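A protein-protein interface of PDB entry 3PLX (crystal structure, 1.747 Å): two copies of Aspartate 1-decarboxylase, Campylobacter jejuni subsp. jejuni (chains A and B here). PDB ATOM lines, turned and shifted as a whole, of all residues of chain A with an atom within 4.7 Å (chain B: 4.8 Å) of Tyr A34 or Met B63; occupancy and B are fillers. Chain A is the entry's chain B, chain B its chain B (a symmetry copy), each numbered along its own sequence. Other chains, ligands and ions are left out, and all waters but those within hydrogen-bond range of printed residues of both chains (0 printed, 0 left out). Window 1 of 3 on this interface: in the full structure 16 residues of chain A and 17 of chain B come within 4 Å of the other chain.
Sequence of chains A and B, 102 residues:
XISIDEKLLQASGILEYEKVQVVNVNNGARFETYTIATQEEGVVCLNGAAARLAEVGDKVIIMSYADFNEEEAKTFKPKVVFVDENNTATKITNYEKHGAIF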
ATOM      1  C   PYR A   1     -29.036 -18.952  29.102  1.00  0.00           C
ATOM      2  OXT PYR A   1     -29.035 -20.121  28.899  1.00  0.00           O
ATOM      3  CA  PYR A   1     -29.634 -18.031  28.043  1.00  0.00           C
ATOM      4  O3  PYR A   1     -30.008 -18.500  27.019  1.00  0.00           O
ATOM      5  CB  PYR A   1     -29.405 -16.524  28.158  1.00  0.00           C
ATOM      6  N   ILE A   2     -28.238 -18.504  30.066  1.00  0.00           N
ATOM      7  CA  ILE A   2     -27.830 -19.375  31.154  1.00  0.00           C
ATOM      8  C   ILE A   2     -28.416 -18.886  32.467  1.00  0.00           C
ATOM      9  O   ILE A   2     -28.093 -17.798  32.945  1.00  0.00           O
ATOM     10  CB  ILE A   2     -26.286 -19.551  31.235  1.00  0.00           C
ATOM     11  CG1 ILE A   2     -25.933 -20.635  32.265  1.00  0.00           C
ATOM     12  CG2 ILE A   2     -25.572 -18.223  31.516  1.00  0.00           C
ATOM     13  CD1 ILE A   2     -24.439 -21.034  32.272  1.00  0.00           C
ATOM     14  N   TYR A  17     -27.929 -10.572  33.540  1.00  0.00           N
ATOM     15  CA  TYR A  17     -27.850 -10.014  32.177  1.00  0.00           C
ATOM     16  C   TYR A  17     -26.431  -9.676  31.719  1.00  0.00           C
ATOM     17  O   TYR A  17     -26.239  -9.189  30.606  1.00  0.00           O
ATOM     18  CB  TYR A  17     -28.827  -8.847  31.959  1.00  0.00           C
ATOM     19  CG  TYR A  17     -30.205  -9.216  32.452  1.00  0.00           C
ATOM     20  CD1 TYR A  17     -30.820 -10.379  32.006  1.00  0.00           C
ATOM     21  CD2 TYR A  17     -30.864  -8.445  33.407  1.00  0.00           C
ATOM     22  CE1 TYR A  17     -32.078 -10.752  32.478  1.00  0.00           C
ATOM     23  CE2 TYR A  17     -32.116  -8.810  33.882  1.00  0.00           C
ATOM     24  CZ  TYR A  17     -32.711  -9.964  33.411  1.00  0.00           C
ATOM     25  OH  TYR A  17     -33.950 -10.343  33.872  1.00  0.00           O
ATOM     26  N   GLU A  18     -25.438  -9.981  32.551  1.00  0.00           N
ATOM     27  CA  GLU A  18     -24.046  -9.788  32.129  1.00  0.00           C
ATOM     28  C   GLU A  18     -23.641 -10.826  31.084  1.00  0.00           C
ATOM     29  O   GLU A  18     -24.057 -11.987  31.150  1.00  0.00           O
ATOM     30  CB  GLU A  18     -23.095  -9.838  33.340  1.00  0.00           C
ATOM     31  CG  GLU A  18     -21.650  -9.476  32.986  1.00  0.00           C
ATOM     32  CD  GLU A  18     -20.791  -9.182  34.213  1.00  0.00           C
ATOM     33  OE1 GLU A  18     -21.327  -9.222  35.341  1.00  0.00           O
ATOM     34  OE2 GLU A  18     -19.581  -8.889  34.046  1.00  0.00           O
ATOM     35  N   LYS A  19     -22.838 -10.404  30.106  1.00  0.00           N
ATOM     36  CA  LYS A  19     -22.270 -11.324  29.132  1.00  0.00           C
ATOM     37  C   LYS A  19     -21.264 -12.250  29.809  1.00  0.00           C
ATOM     38  O   LYS A  19     -20.406 -11.801  30.574  1.00  0.00           O
ATOM     39  CB  LYS A  19     -21.565 -10.548  28.024  1.00  0.00           C
ATOM     40  CG  LYS A  19     -21.001 -11.417  26.904  1.00  0.00           C
ATOM     41  CD  LYS A  19     -20.390 -10.515  25.831  1.00  0.00           C
ATOM     42  CE  LYS A  19     -20.072 -11.265  24.558  1.00  0.00           C
ATOM     43  NZ  LYS A  19     -19.376 -10.365  23.573  1.00  0.00           N
ATOM     44  N   VAL A  20     -21.372 -13.544  29.538  1.00  0.00           N
ATOM     45  CA  VAL A  20     -20.412 -14.501  30.092  1.00  0.00           C
ATOM     46  C   VAL A  20     -19.913 -15.436  29.004  1.00  0.00           C
ATOM     47  O   VAL A  20     -20.627 -15.727  28.031  1.00  0.00           O
ATOM     48  CB  VAL A  20     -21.011 -15.339  31.251  1.00  0.00           C
ATOM     49  CG1 VAL A  20     -21.241 -14.467  32.484  1.00  0.00           C
ATOM     50  CG2 VAL A  20     -22.314 -16.030  30.810  1.00  0.00           C
ATOM     51  N   THR A  33     -22.859 -16.064  26.118  1.00  0.00           N
ATOM     52  CA  THR A  33     -24.280 -15.821  26.293  1.00  0.00           C
ATOM     53  C   THR A  33     -24.422 -14.779  27.396  1.00  0.00           C
ATOM     54  O   THR A  33     -23.455 -14.097  27.711  1.00  0.00           O
ATOM     55  CB  THR A  33     -25.041 -17.132  26.593  1.00  0.00           C
ATOM     56  OG1 THR A  33     -26.453 -16.893  26.523  1.00  0.00           O
ATOM     57  CG2 THR A  33     -24.633 -17.727  27.947  1.00  0.00           C
ATOM     58  N   TYR A  34     -25.618 -14.622  27.953  1.00  0.00           N
ATOM     59  CA  TYR A  34     -25.799 -13.708  29.080  1.00  0.00           C
ATOM     60  C   TYR A  34     -26.488 -14.458  30.212  1.00  0.00           C
ATOM     61  O   TYR A  34     -27.120 -15.488  29.984  1.00  0.00           O
ATOM     62  CB  TYR A  34     -26.637 -12.493  28.673  1.00  0.00           C
ATOM     63  CG  TYR A  34     -28.044 -12.838  28.255  1.00  0.00           C
ATOM     64  CD1 TYR A  34     -29.076 -12.859  29.185  1.00  0.00           C
ATOM     65  CD2 TYR A  34     -28.341 -13.157  26.926  1.00  0.00           C
ATOM     66  CE1 TYR A  34     -30.378 -13.184  28.810  1.00  0.00           C
ATOM     67  CE2 TYR A  34     -29.637 -13.479  26.543  1.00  0.00           C
ATOM     68  CZ  TYR A  34     -30.650 -13.483  27.489  1.00  0.00           C
ATOM     69  OH  TYR A  34     -31.946 -13.802  27.123  1.00  0.00           O
ATOM     70  N   THR A  35     -26.387 -13.935  31.430  1.00  0.00           N
ATOM     71  CA  THR A  35     -26.943 -14.656  32.564  1.00  0.00           C
ATOM     72  C   THR A  35     -28.383 -14.262  32.847  1.00  0.00           C
ATOM     73  O   THR A  35     -28.807 -13.133  32.579  1.00  0.00           O
ATOM     74  CB  THR A  35     -26.131 -14.393  33.834  1.00  0.00           C
ATOM     75  OG1 THR A  35     -26.263 -13.011  34.194  1.00  0.00           O
ATOM     76  CG2 THR A  35     -24.648 -14.716  33.602  1.00  0.00           C
ATOM     77  N   ILE A  36     -29.123 -15.206  33.413  1.00  0.00           N
ATOM     78  CA  ILE A  36     -30.421 -14.921  34.004  1.00  0.00           C
ATOM     79  C   ILE A  36     -30.365 -15.440  35.432  1.00  0.00           C
ATOM     80  O   ILE A  36     -29.876 -16.532  35.661  1.00  0.00           O
ATOM     81  CB  ILE A  36     -31.543 -15.650  33.248  1.00  0.00           C
ATOM     82  CG1 ILE A  36     -31.606 -15.152  31.801  1.00  0.00           C
ATOM     83  CG2 ILE A  36     -32.885 -15.424  33.950  1.00  0.00           C
ATOM     84  CD1 ILE A  36     -32.462 -16.017  30.873  1.00  0.00           C
ATOM     85  N   LYS B  19     -23.482  -4.524  15.547  1.00  0.00           N
ATOM     86  CA  LYS B  19     -23.018  -5.893  15.717  1.00  0.00           C
ATOM     87  C   LYS B  19     -24.031  -6.693  16.531  1.00  0.00           C
ATOM     88  O   LYS B  19     -24.508  -6.234  17.573  1.00  0.00           O
ATOM     89  CB  LYS B  19     -21.675  -5.906  16.441  1.00  0.00           C
ATOM     90  CG  LYS B  19     -21.057  -7.292  16.601  1.00  0.00           C
ATOM     91  CD  LYS B  19     -19.691  -7.156  17.272  1.00  0.00           C
ATOM     92  CE  LYS B  19     -18.885  -8.432  17.208  1.00  0.00           C
ATOM     93  NZ  LYS B  19     -17.597  -8.284  17.971  1.00  0.00           N
ATOM     94  N   VAL B  20     -24.367  -7.884  16.056  1.00  0.00           N
ATOM     95  CA  VAL B  20     -25.284  -8.749  16.801  1.00  0.00           C
ATOM     96  C   VAL B  20     -24.724 -10.160  16.886  1.00  0.00           C
ATOM     97  O   VAL B  20     -23.989 -10.613  15.995  1.00  0.00           O
ATOM     98  CB  VAL B  20     -26.699  -8.798  16.170  1.00  0.00           C
ATOM     99  CG1 VAL B  20     -27.414  -7.459  16.344  1.00  0.00           C
ATOM    100  CG2 VAL B  20     -26.622  -9.195  14.684  1.00  0.00           C
ATOM    101  N   GLN B  21     -25.053 -10.838  17.980  1.00  0.00           N
ATOM    102  CA  GLN B  21     -24.826 -12.270  18.086  1.00  0.00           C
ATOM    103  C   GLN B  21     -26.118 -12.959  17.666  1.00  0.00           C
ATOM    104  O   GLN B  21     -27.204 -12.574  18.112  1.00  0.00           O
ATOM    105  CB  GLN B  21     -24.503 -12.648  19.531  1.00  0.00           C
ATOM    106  CG  GLN B  21     -24.292 -14.152  19.686  1.00  0.00           C
ATOM    107  CD  GLN B  21     -24.028 -14.573  21.128  1.00  0.00           C
ATOM    108  OE1 GLN B  21     -23.398 -15.604  21.381  1.00  0.00           O
ATOM    109  NE2 GLN B  21     -24.530 -13.799  22.067  1.00  0.00           N
ATOM    110  N   VAL B  23     -27.943 -16.748  17.317  1.00  0.00           N
ATOM    111  CA  VAL B  23     -27.822 -18.173  17.624  1.00  0.00           C
ATOM    112  C   VAL B  23     -29.037 -18.892  17.065  1.00  0.00           C
ATOM    113  O   VAL B  23     -30.139 -18.348  17.032  1.00  0.00           O
ATOM    114  CB  VAL B  23     -27.625 -18.450  19.141  1.00  0.00           C
ATOM    115  CG1 VAL B  23     -26.405 -17.682  19.660  1.00  0.00           C
ATOM    116  CG2 VAL B  23     -28.862 -18.049  19.921  1.00  0.00           C
ATOM    117  N   ILE B  61     -32.208 -16.481  17.717  1.00  0.00           N
ATOM    118  CA  ILE B  61     -32.267 -15.472  18.756  1.00  0.00           C
ATOM    119  C   ILE B  61     -31.161 -14.476  18.412  1.00  0.00           C
ATOM    120  O   ILE B  61     -30.014 -14.872  18.188  1.00  0.00           O
ATOM    121  CB  ILE B  61     -32.057 -16.106  20.146  1.00  0.00           C
ATOM    122  CG1 ILE B  61     -33.185 -17.117  20.418  1.00  0.00           C
ATOM    123  CG2 ILE B  61     -32.017 -15.029  21.234  1.00  0.00           C
ATOM    124  CD1 ILE B  61     -32.965 -17.982  21.630  1.00  0.00           C
ATOM    125  N   ILE B  62     -31.526 -13.196  18.323  1.00  0.00           N
ATOM    126  CA  ILE B  62     -30.624 -12.146  17.854  1.00  0.00           C
ATOM    127  C   ILE B  62     -30.391 -11.172  19.006  1.00  0.00           C
ATOM    128  O   ILE B  62     -31.352 -10.596  19.540  1.00  0.00           O
ATOM    129  CB  ILE B  62     -31.252 -11.381  16.667  1.00  0.00           C
ATOM    130  CG1 ILE B  62     -31.521 -12.327  15.488  1.00  0.00           C
ATOM    131  CG2 ILE B  62     -30.341 -10.239  16.226  1.00  0.00           C
ATOM    132  CD1 ILE B  62     -32.667 -11.863  14.575  1.00  0.00           C
ATOM    133  N   MET B  63     -29.133 -11.001  19.410  1.00  0.00           N
ATOM    134  CA  MET B  63     -28.825 -10.265  20.635  1.00  0.00           C
ATOM    135  C   MET B  63     -27.827  -9.157  20.351  1.00  0.00           C
ATOM    136  O   MET B  63     -26.910  -9.342  19.555  1.00  0.00           O
ATOM    137  CB  MET B  63     -28.209 -11.212  21.677  1.00  0.00           C
ATOM    138  CG  MET B  63     -29.172 -12.267  22.191  1.00  0.00           C
ATOM    139  SD  MET B  63     -28.364 -13.648  23.038  1.00  0.00           S
ATOM    140  CE  MET B  63     -27.728 -14.573  21.630  1.00  0.00           C
ATOM    141  N   SER B  64     -28.016  -8.006  20.993  1.00  0.00           N
ATOM    142  CA  SER B  64     -26.986  -6.974  20.975  1.00  0.00           C
ATOM    143  C   SER B  64     -26.524  -6.747  22.396  1.00  0.00           C
ATOM    144  O   SER B  64     -27.288  -6.967  23.340  1.00  0.00           O
ATOM    145  CB  SER B  64     -27.511  -5.665  20.367  1.00  0.00           C
ATOM    146  OG  SER B  64     -28.405  -5.021  21.255  1.00  0.00           O
ATOM    147  N   TYR B  65     -25.272  -6.316  22.549  1.00  0.00           N
ATOM    148  CA  TYR B  65     -24.675  -6.121  23.861  1.00  0.00           C
ATOM    149  C   TYR B  65     -24.129  -4.720  23.929  1.00  0.00           C
ATOM    150  O   TYR B  65     -23.864  -4.099  22.902  1.00  0.00           O
ATOM    151  CB  TYR B  65     -23.504  -7.091  24.038  1.00  0.00           C
ATOM    152  CG  TYR B  65     -23.946  -8.520  24.148  1.00  0.00           C
ATOM    153  CD1 TYR B  65     -24.187  -9.088  25.398  1.00  0.00           C
ATOM    154  CD2 TYR B  65     -24.146  -9.300  23.017  1.00  0.00           C
ATOM    155  CE1 TYR B  65     -24.611 -10.387  25.516  1.00  0.00           C
ATOM    156  CE2 TYR B  65     -24.573 -10.618  23.126  1.00  0.00           C
ATOM    157  CZ  TYR B  65     -24.804 -11.151  24.385  1.00  0.00           C
ATOM    158  OH  TYR B  65     -25.213 -12.463  24.523  1.00  0.00           O
ATOM    159  N   TYR B  95     -36.610  -6.902  30.623  1.00  0.00           N
ATOM    160  CA  TYR B  95     -36.372  -7.897  31.653  1.00  0.00           C
ATOM    161  C   TYR B  95     -36.511  -7.277  33.034  1.00  0.00           C
ATOM    162  O   TYR B  95     -36.039  -6.165  33.275  1.00  0.00           O
ATOM    163  CB  TYR B  95     -34.952  -8.428  31.532  1.00  0.00           C
ATOM    164  CG  TYR B  95     -34.787  -9.690  30.726  1.00  0.00           C
ATOM    165  CD1 TYR B  95     -33.836  -9.761  29.719  1.00  0.00           C
ATOM    166  CD2 TYR B  95     -35.547 -10.823  30.994  1.00  0.00           C
ATOM    167  CE1 TYR B  95     -33.648 -10.912  28.987  1.00  0.00           C
ATOM    168  CE2 TYR B  95     -35.367 -11.992  30.259  1.00  0.00           C
ATOM    169  CZ  TYR B  95     -34.412 -12.026  29.258  1.00  0.00           C
ATOM    170  OH  TYR B  95     -34.210 -13.171  28.523  1.00  0.00           O
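The backbone carbonyl oxygen (O) of Thr A35 is in hydrogen-bond range of the backbone NH (N) of Tyr A17 (2.9 Å).
O of Gln B21 sits at hydrogen-bond distance from N of Met B63 (2.8 Å).
OH of Tyr B65 lies within hydrogen-bond range of NE2 of Gln B21 (2.9 Å).
The side-chain sulfur (SD) of Met B63 is in hydrogen-bond range of the side-chain hydroxyl (OH) of Tyr B65 (3.7 Å).
The backbone carbonyl oxygen (O) of Thr A33 sits at hydrogen-bond distance from the backbone NH (N) of Val A20, 2.8 Å away.
N of Ile A2 is in hydrogen-bond range of O of Tyr A34 (3.2 Å).
Of the 10 printed residues of chain B, 3 touch a printed residue of chain A.
Printed residues of chain B that touch a printed residue of chain A: Met B63, Tyr B65 and Tyr B95.
Of the 10 printed residues of chain A, 4 touch a printed residue of chain B.
Positions printed for both chains: 19 and 20.
Of the 5 pairs that touch across the chains among the printed residues, none has its exchanged pair printed and touching as well.
Tyr A17 touches Tyr B95.
Tyr B65 touches Lys A19.
Thr A33 touches Tyr B65.
Tyr A34 touches Met B63 (CE2 to SD, 3.7 Å).
OH of Tyr A34 lies within hydrogen-bond range of OH of Tyr B95 (2.7 Å).
Of the printed residues of chain B, Tyr A17 touches Tyr B95 (3.2 Å).
Printed residues of chain B within 4 Å of Lys A19: Tyr B65 (3.9 Å).
Printed residues of chain B within 4 Å of Thr A33: Tyr B65 (3.8 Å).
Of the printed residues of chain A, Met B63 touches Tyr A34 (3.7 Å).
Of the printed residues of chain A, Tyr B65 touches Lys A19 and Thr A33.
The nearest printed residue of chain A that does not touch Met B63 is Thr A33 (5.1 Å).
The nearest printed residue of chain A that does not touch Tyr B65 is Tyr A34 (4.01 Å).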
